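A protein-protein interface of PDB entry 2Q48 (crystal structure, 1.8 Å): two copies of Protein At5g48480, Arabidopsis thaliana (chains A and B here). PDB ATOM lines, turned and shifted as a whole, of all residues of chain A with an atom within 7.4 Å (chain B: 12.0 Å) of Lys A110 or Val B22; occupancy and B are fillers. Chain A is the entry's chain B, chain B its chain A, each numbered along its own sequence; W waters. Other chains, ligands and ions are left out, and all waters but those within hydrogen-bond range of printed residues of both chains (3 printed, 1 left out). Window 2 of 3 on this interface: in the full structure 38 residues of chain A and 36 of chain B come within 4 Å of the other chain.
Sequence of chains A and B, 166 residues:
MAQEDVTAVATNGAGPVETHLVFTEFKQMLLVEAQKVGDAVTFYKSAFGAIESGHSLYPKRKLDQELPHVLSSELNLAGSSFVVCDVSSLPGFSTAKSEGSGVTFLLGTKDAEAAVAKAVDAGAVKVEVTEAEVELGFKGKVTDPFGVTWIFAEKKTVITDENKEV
The side-chain hydroxyl (OG1) of Thr A109 lies within hydrogen-bond range of the backbone carbonyl oxygen (O) of Val B22, at 3.4 Å.
N of Thr B24 lies within hydrogen-bond range of O of Gly A108 (2.5 Å).
N of Gly A108 sits at hydrogen-bond distance from O of Glu B25 (3.3 Å).
OE2 of Glu B25 is in salt-bridge range of NZ of Lys B27 (3.2 Å).
The backbone carbonyl oxygen (O) of Leu A107 lies within hydrogen-bond range of the backbone NH (N) of Ala A153, 3.0 Å away.
The side-chain hydroxyl (OG1) of Thr A109 is in hydrogen-bond range of the backbone NH (N) of Asp A111.
The backbone NH (N) of Thr A109 is in hydrogen-bond range of the backbone carbonyl oxygen (O) of Ala A153, at 2.9 Å.
OD1 of Asp A111 lies within hydrogen-bond range of N of Ala A114 (2.9 Å).
Among the printed residues, merely in contact across the chains: Gly A108 with Phe B23 (3.2 Å), Leu A77 with Phe B26 (3.2 Å), Leu A107 with Glu B25 (3.3 Å), Phe A48 with Phe B23 (3.3 Å), Lys A110 with Val B22 (3.4 Å), Leu A107 with Phe B26 (3.5 Å), Ala A78 with Phe B26 (3.5 Å), Thr A109 with Leu B21 (3.5 Å), Ala A115 with Leu B21 (3.6 Å), Ala A78 with Glu B25 (3.7 Å), Thr A109 with Thr B24 (3.8 Å), Lys A118 with Leu B21 (3.8 Å), Thr A109 with Phe B23 (3.8 Å), Ala A115 with Phe B23 (3.9 Å), Ala A114 with Leu B21 (3.9 Å), Ala A78 with Phe B23 (3.9 Å) and Leu A107 with Phe B23 (3.9 Å).
Of chain B, only Val B22 (3.4 Å) comes within 4 Å of Lys A110.
Of the printed residues of chain A, Val B22 touches Thr A109 and Lys A110.
Of chain B, only Leu B21, Val B22, Phe B23 and Thr B24 come within 4 Å of Thr A109.
No residue of chain B comes within 4 Å of Asp A111.
No residue of chain B comes within 4 Å of Ala A112.
No residue of chain B comes within 4 Å of Glu A154.
Of the printed residues of chain B, Phe A48 touches Phe B23.
Of the printed residues of chain A, Glu B25 touches Ala A78 (3.7 Å), Leu A107 (3.3 Å) and Gly A108 (3.3 Å).
Of the printed residues of chain B, Ala A114 touches Leu B21.
Printed residues of chain B within 4 Å of Leu A77: Phe B26.
Ala A153 touches none of the printed residues of chain B.
The nearest residue of chain A that does not touch Val B22 is Gly A108 (4.4 Å).
Printed residues of chain A that touch a printed residue of chain B: Phe A48, Leu A77, Ala A78, Leu A107, Gly A108, Thr A109, Lys A110, Ala A114, Ala A115 and Lys A118.
Hydrophobic or aromatic side chains of chain A that line the printed part of chain B: Phe A48, Ala A78, Leu A107 and Ala A115.
Along chain A the printed residues that touch a printed residue of chain B span positions 48 to 118.
Printed residues of chain B that touch a printed residue of chain A: Leu B21, Val B22, Phe B23, Thr B24, Glu B25 and Phe B26.
Hydrophobic or aromatic side chains of chain B that line the printed part of chain A: Leu B21, Val B22, Phe B23 and Phe B26.
Among the printed residues, no Asp or Glu carboxylate lies within 4 Å of a Lys or Arg side-chain nitrogen of the other chain.
No position is printed for both chains.
Water W3 lies within hydrogen-bond range of O of Ala A78 and O of Phe B26.
Water W2 lies within hydrogen-bond range of the side-chain hydroxyl (OG1) of Thr B24 (2.9 Å) and the backbone carbonyl oxygen (O) of Thr A109 (3.4 Å).
Water W1 lies within hydrogen-bond range of the backbone NH (N) of Leu B21 (3.0 Å) and the side-chain amino group (NZ) of Lys A118 (3.5 Å).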
ATOM      1  N   PHE A  48     -17.506  -1.027  26.227  1.00  0.00           N
ATOM      2  CA  PHE A  48     -17.881  -1.674  24.985  1.00  0.00           C
ATOM      3  C   PHE A  48     -18.596  -3.001  25.104  1.00  0.00           C
ATOM      4  O   PHE A  48     -18.982  -3.583  24.087  1.00  0.00           O
ATOM      5  CB  PHE A  48     -16.608  -1.892  24.131  1.00  0.00           C
ATOM      6  CG  PHE A  48     -15.759  -0.655  23.962  1.00  0.00           C
ATOM      7  CD1 PHE A  48     -16.321   0.521  23.487  1.00  0.00           C
ATOM      8  CD2 PHE A  48     -14.387  -0.666  24.288  1.00  0.00           C
ATOM      9  CE1 PHE A  48     -15.563   1.658  23.337  1.00  0.00           C
ATOM     10  CE2 PHE A  48     -13.626   0.466  24.136  1.00  0.00           C
ATOM     11  CZ  PHE A  48     -14.207   1.637  23.662  1.00  0.00           C
ATOM     12  N   LEU A  77     -14.895  -9.086  21.241  1.00  0.00           N
ATOM     13  CA  LEU A  77     -15.712  -7.939  20.966  1.00  0.00           C
ATOM     14  C   LEU A  77     -16.038  -7.886  19.506  1.00  0.00           C
ATOM     15  O   LEU A  77     -15.150  -7.887  18.639  1.00  0.00           O
ATOM     16  CB  LEU A  77     -14.954  -6.632  21.343  1.00  0.00           C
ATOM     17  CG  LEU A  77     -15.626  -5.269  21.107  1.00  0.00           C
ATOM     18  CD1 LEU A  77     -16.954  -5.134  21.914  1.00  0.00           C
ATOM     19  CD2 LEU A  77     -14.632  -4.163  21.539  1.00  0.00           C
ATOM     20  N   ALA A  78     -17.329  -7.854  19.247  1.00  0.00           N
ATOM     21  CA  ALA A  78     -17.824  -7.692  17.888  1.00  0.00           C
ATOM     22  C   ALA A  78     -17.190  -8.624  16.878  1.00  0.00           C
ATOM     23  O   ALA A  78     -16.757  -8.168  15.782  1.00  0.00           O
ATOM     24  CB  ALA A  78     -17.640  -6.190  17.450  1.00  0.00           C
ATOM     25  N   LEU A 107     -14.892   0.859  15.485  1.00  0.00           N
ATOM     26  CA  LEU A 107     -16.060   0.128  15.964  1.00  0.00           C
ATOM     27  C   LEU A 107     -17.274   0.761  15.284  1.00  0.00           C
ATOM     28  O   LEU A 107     -17.533   1.938  15.512  1.00  0.00           O
ATOM     29  CB  LEU A 107     -16.266   0.301  17.472  1.00  0.00           C
ATOM     30  CG  LEU A 107     -15.390  -0.567  18.387  1.00  0.00           C
ATOM     31  CD1 LEU A 107     -15.714  -0.310  19.844  1.00  0.00           C
ATOM     32  CD2 LEU A 107     -15.657  -2.032  17.998  1.00  0.00           C
ATOM     33  N   GLY A 108     -17.995  -0.011  14.465  1.00  0.00           N
ATOM     34  CA  GLY A 108     -19.206   0.504  13.807  1.00  0.00           C
ATOM     35  C   GLY A 108     -20.401   0.374  14.739  1.00  0.00           C
ATOM     36  O   GLY A 108     -20.577  -0.660  15.369  1.00  0.00           O
ATOM     37  N   THR A 109     -21.242   1.401  14.822  1.00  0.00           N
ATOM     38  CA  THR A 109     -22.365   1.306  15.731  1.00  0.00           C
ATOM     39  C   THR A 109     -23.555   2.077  15.227  1.00  0.00           C
ATOM     40  O   THR A 109     -23.432   2.911  14.328  1.00  0.00           O
ATOM     41  CB  THR A 109     -21.998   1.865  17.086  1.00  0.00           C
ATOM     42  OG1 THR A 109     -23.157   1.866  17.926  1.00  0.00           O
ATOM     43  CG2 THR A 109     -21.469   3.270  16.955  1.00  0.00           C
ATOM     44  N   LYS A 110     -24.718   1.801  15.799  1.00  0.00           N
ATOM     45  CA  LYS A 110     -25.885   2.531  15.359  1.00  0.00           C
ATOM     46  C   LYS A 110     -25.907   3.965  15.873  1.00  0.00           C
ATOM     47  O   LYS A 110     -26.355   4.871  15.160  1.00  0.00           O
ATOM     48  CB  LYS A 110     -27.147   1.793  15.798  1.00  0.00           C
ATOM     49  CG  LYS A 110     -27.212   0.385  15.248  1.00  0.00           C
ATOM     50  CD  LYS A 110     -28.456  -0.326  15.717  1.00  0.00           C
ATOM     51  CE  LYS A 110     -28.474  -1.775  15.241  1.00  0.00           C
ATOM     52  NZ  LYS A 110     -27.251  -2.528  15.690  1.00  0.00           N
ATOM     53  N   ASP A 111     -25.432   4.184  17.098  1.00  0.00           N
ATOM     54  CA  ASP A 111     -25.451   5.527  17.682  1.00  0.00           C
ATOM     55  C   ASP A 111     -24.071   5.888  18.219  1.00  0.00           C
ATOM     56  O   ASP A 111     -23.706   5.501  19.334  1.00  0.00           O
ATOM     57  CB  ASP A 111     -26.490   5.574  18.827  1.00  0.00           C
ATOM     58  CG  ASP A 111     -26.696   6.984  19.412  1.00  0.00           C
ATOM     59  OD1 ASP A 111     -25.783   7.832  19.285  1.00  0.00           O
ATOM     60  OD2 ASP A 111     -27.779   7.232  20.018  1.00  0.00           O
ATOM     61  N   ALA A 112     -23.323   6.669  17.451  1.00  0.00           N
ATOM     62  CA  ALA A 112     -21.978   7.037  17.870  1.00  0.00           C
ATOM     63  C   ALA A 112     -21.930   7.890  19.134  1.00  0.00           C
ATOM     64  O   ALA A 112     -21.165   7.595  20.056  1.00  0.00           O
ATOM     65  CB  ALA A 112     -21.258   7.717  16.735  1.00  0.00           C
ATOM     66  N   GLU A 113     -22.763   8.940  19.225  1.00  0.00           N
ATOM     67  CA  GLU A 113     -22.689   9.768  20.429  1.00  0.00           C
ATOM     68  C   GLU A 113     -23.019   8.942  21.681  1.00  0.00           C
ATOM     69  O   GLU A 113     -22.437   9.139  22.748  1.00  0.00           O
ATOM     70  CB  GLU A 113     -23.621  11.004  20.311  1.00  0.00           C
ATOM     71  CG  GLU A 113     -23.436  11.974  21.470  1.00  0.00           C
ATOM     72  CD  GLU A 113     -21.964  12.221  21.796  1.00  0.00           C
ATOM     73  OE1 GLU A 113     -21.251  12.847  20.966  1.00  0.00           O
ATOM     74  OE2 GLU A 113     -21.526  11.775  22.881  1.00  0.00           O
ATOM     75  N   ALA A 114     -23.951   8.010  21.551  1.00  0.00           N
ATOM     76  CA  ALA A 114     -24.294   7.136  22.674  1.00  0.00           C
ATOM     77  C   ALA A 114     -23.079   6.314  23.107  1.00  0.00           C
ATOM     78  O   ALA A 114     -22.823   6.123  24.299  1.00  0.00           O
ATOM     79  CB  ALA A 114     -25.387   6.197  22.272  1.00  0.00           C
ATOM     80  N   ALA A 115     -22.348   5.798  22.128  1.00  0.00           N
ATOM     81  CA  ALA A 115     -21.160   4.971  22.453  1.00  0.00           C
ATOM     82  C   ALA A 115     -20.066   5.855  23.041  1.00  0.00           C
ATOM     83  O   ALA A 115     -19.323   5.428  23.921  1.00  0.00           O
ATOM     84  CB  ALA A 115     -20.650   4.230  21.193  1.00  0.00           C
ATOM     85  N   LYS A 118     -21.065   6.445  26.619  1.00  0.00           N
ATOM     86  CA  LYS A 118     -21.020   5.167  27.298  1.00  0.00           C
ATOM     87  C   LYS A 118     -19.570   4.875  27.652  1.00  0.00           C
ATOM     88  O   LYS A 118     -19.320   4.332  28.696  1.00  0.00           O
ATOM     89  CB  LYS A 118     -21.590   4.044  26.412  1.00  0.00           C
ATOM     90  CG  LYS A 118     -21.728   2.677  27.113  1.00  0.00           C
ATOM     91  CD  LYS A 118     -22.262   1.534  26.159  1.00  0.00           C
ATOM     92  CE  LYS A 118     -21.735   0.111  26.563  1.00  0.00           C
ATOM     93  NZ  LYS A 118     -22.032  -1.031  25.583  1.00  0.00           N
ATOM     94  N   ALA A 153     -17.931   4.475  13.907  1.00  0.00           N
ATOM     95  CA  ALA A 153     -18.527   4.731  12.604  1.00  0.00           C
ATOM     96  C   ALA A 153     -20.036   4.671  12.761  1.00  0.00           C
ATOM     97  O   ALA A 153     -20.537   4.016  13.667  1.00  0.00           O
ATOM     98  CB  ALA A 153     -18.043   3.689  11.562  1.00  0.00           C
ATOM     99  N   GLU A 154     -20.758   5.352  11.870  1.00  0.00           N
ATOM    100  CA  GLU A 154     -22.208   5.397  11.952  1.00  0.00           C
ATOM    101  C   GLU A 154     -22.811   5.969  10.676  1.00  0.00           C
ATOM    102  O   GLU A 154     -23.716   5.334  10.082  1.00  0.00           O
ATOM    103  CB  GLU A 154     -22.612   6.279  13.125  1.00  0.00           C
ATOM    104  CG  GLU A 154     -24.075   6.355  13.380  1.00  0.00           C
ATOM    105  CD  GLU A 154     -24.433   7.593  14.162  1.00  0.00           C
ATOM    106  OE1 GLU A 154     -24.432   8.688  13.565  1.00  0.00           O
ATOM    107  OE2 GLU A 154     -24.705   7.474  15.369  1.00  0.00           O
ATOM    108  N   HIS B  20     -29.415  -1.396  25.506  1.00  0.00           N
ATOM    109  CA  HIS B  20     -28.449  -2.361  24.897  1.00  0.00           C
ATOM    110  C   HIS B  20     -27.761  -1.799  23.644  1.00  0.00           C
ATOM    111  O   HIS B  20     -28.363  -1.730  22.573  1.00  0.00           O
ATOM    112  CB  HIS B  20     -29.181  -3.663  24.560  1.00  0.00           C
ATOM    113  CG  HIS B  20     -29.674  -4.400  25.770  1.00  0.00           C
ATOM    114  ND1 HIS B  20     -30.485  -3.814  26.720  1.00  0.00           N
ATOM    115  CD2 HIS B  20     -29.428  -5.655  26.209  1.00  0.00           C
ATOM    116  CE1 HIS B  20     -30.713  -4.676  27.694  1.00  0.00           C
ATOM    117  NE2 HIS B  20     -30.084  -5.801  27.410  1.00  0.00           N
ATOM    118  N   LEU B  21     -26.505  -1.390  23.775  1.00  0.00           N
ATOM    119  CA  LEU B  21     -25.777  -0.840  22.630  1.00  0.00           C
ATOM    120  C   LEU B  21     -24.838  -1.917  22.082  1.00  0.00           C
ATOM    121  O   LEU B  21     -24.110  -2.559  22.830  1.00  0.00           O
ATOM    122  CB  LEU B  21     -25.000   0.406  23.065  1.00  0.00           C
ATOM    123  CG  LEU B  21     -24.225   1.198  22.017  1.00  0.00           C
ATOM    124  CD1 LEU B  21     -25.120   1.595  20.852  1.00  0.00           C
ATOM    125  CD2 LEU B  21     -23.661   2.450  22.689  1.00  0.00           C
ATOM    126  N   VAL B  22     -24.873  -2.128  20.776  1.00  0.00           N
ATOM    127  CA  VAL B  22     -24.042  -3.163  20.149  1.00  0.00           C
ATOM    128  C   VAL B  22     -23.208  -2.541  19.049  1.00  0.00           C
ATOM    129  O   VAL B  22     -23.567  -1.464  18.519  1.00  0.00           O
ATOM    130  CB  VAL B  22     -24.944  -4.266  19.542  1.00  0.00           C
ATOM    131  CG1 VAL B  22     -25.866  -3.645  18.557  1.00  0.00           C
ATOM    132  CG2 VAL B  22     -24.109  -5.366  18.910  1.00  0.00           C
ATOM    133  N   PHE B  23     -22.105  -3.209  18.721  1.00  0.00           N
ATOM    134  CA  PHE B  23     -21.184  -2.761  17.675  1.00  0.00           C
ATOM    135  C   PHE B  23     -21.256  -3.667  16.474  1.00  0.00           C
ATOM    136  O   PHE B  23     -21.250  -4.875  16.619  1.00  0.00           O
ATOM    137  CB  PHE B  23     -19.766  -2.697  18.259  1.00  0.00           C
ATOM    138  CG  PHE B  23     -19.679  -1.734  19.411  1.00  0.00           C
ATOM    139  CD1 PHE B  23     -19.761  -0.370  19.182  1.00  0.00           C
ATOM    140  CD2 PHE B  23     -19.606  -2.184  20.709  1.00  0.00           C
ATOM    141  CE1 PHE B  23     -19.768   0.531  20.237  1.00  0.00           C
ATOM    142  CE2 PHE B  23     -19.612  -1.284  21.791  1.00  0.00           C
ATOM    143  CZ  PHE B  23     -19.695   0.094  21.538  1.00  0.00           C
ATOM    144  N   THR B  24     -21.351  -3.065  15.296  1.00  0.00           N
ATOM    145  CA  THR B  24     -21.491  -3.792  14.049  1.00  0.00           C
ATOM    146  C   THR B  24     -20.210  -4.398  13.485  1.00  0.00           C
ATOM    147  O   THR B  24     -20.252  -5.092  12.451  1.00  0.00           O
ATOM    148  CB  THR B  24     -22.182  -2.905  12.965  1.00  0.00           C
ATOM    149  OG1 THR B  24     -21.416  -1.719  12.735  1.00  0.00           O
ATOM    150  CG2 THR B  24     -23.595  -2.490  13.432  1.00  0.00           C
ATOM    151  N   GLU B  25     -19.079  -4.129  14.148  1.00  0.00           N
ATOM    152  CA  GLU B  25     -17.805  -4.694  13.724  1.00  0.00           C
ATOM    153  C   GLU B  25     -16.679  -4.083  14.553  1.00  0.00           C
ATOM    154  O   GLU B  25     -16.865  -3.012  15.115  1.00  0.00           O
ATOM    155  CB  GLU B  25     -17.564  -4.438  12.229  1.00  0.00           C
ATOM    156  CG  GLU B  25     -17.460  -2.985  11.828  1.00  0.00           C
ATOM    157  CD  GLU B  25     -17.325  -2.822  10.325  1.00  0.00           C
ATOM    158  OE1 GLU B  25     -18.135  -3.446   9.603  1.00  0.00           O
ATOM    159  OE2 GLU B  25     -16.430  -2.080   9.859  1.00  0.00           O
ATOM    160  N   PHE B  26     -15.545  -4.778  14.619  1.00  0.00           N
ATOM    161  CA  PHE B  26     -14.386  -4.324  15.384  1.00  0.00           C
ATOM    162  C   PHE B  26     -13.112  -4.621  14.603  1.00  0.00           C
ATOM    163  O   PHE B  26     -12.753  -5.783  14.390  1.00  0.00           O
ATOM    164  CB  PHE B  26     -14.394  -5.019  16.757  1.00  0.00           C
ATOM    165  CG  PHE B  26     -13.093  -4.903  17.557  1.00  0.00           C
ATOM    166  CD1 PHE B  26     -12.434  -3.665  17.739  1.00  0.00           C
ATOM    167  CD2 PHE B  26     -12.575  -6.022  18.178  1.00  0.00           C
ATOM    168  CE1 PHE B  26     -11.281  -3.584  18.537  1.00  0.00           C
ATOM    169  CE2 PHE B  26     -11.429  -5.956  18.972  1.00  0.00           C
ATOM    170  CZ  PHE B  26     -10.773  -4.729  19.152  1.00  0.00           C
ATOM    171  N   LYS B  27     -12.450  -3.562  14.169  1.00  0.00           N
ATOM    172  CA  LYS B  27     -11.221  -3.691  13.391  1.00  0.00           C
ATOM    173  C   LYS B  27     -10.083  -2.933  14.045  1.00  0.00           C
ATOM    174  O   LYS B  27     -10.305  -1.908  14.741  1.00  0.00           O
ATOM    175  CB  LYS B  27     -11.425  -3.165  11.975  1.00  0.00           C
ATOM    176  CG  LYS B  27     -12.513  -3.918  11.195  1.00  0.00           C
ATOM    177  CD  LYS B  27     -12.679  -3.367   9.788  1.00  0.00           C
ATOM    178  CE  LYS B  27     -13.244  -1.964   9.797  1.00  0.00           C
ATOM    179  NZ  LYS B  27     -13.639  -1.529   8.411  1.00  0.00           N
HETATM  180  O   HOH W   1     -25.380  -0.929  26.568  1.00  0.00           O
HETATM  181  O   HOH W   2     -23.559   0.175  12.329  1.00  0.00           O
HETATM  182  O   HOH W   3     -14.846  -8.374  13.962  1.00  0.00           O
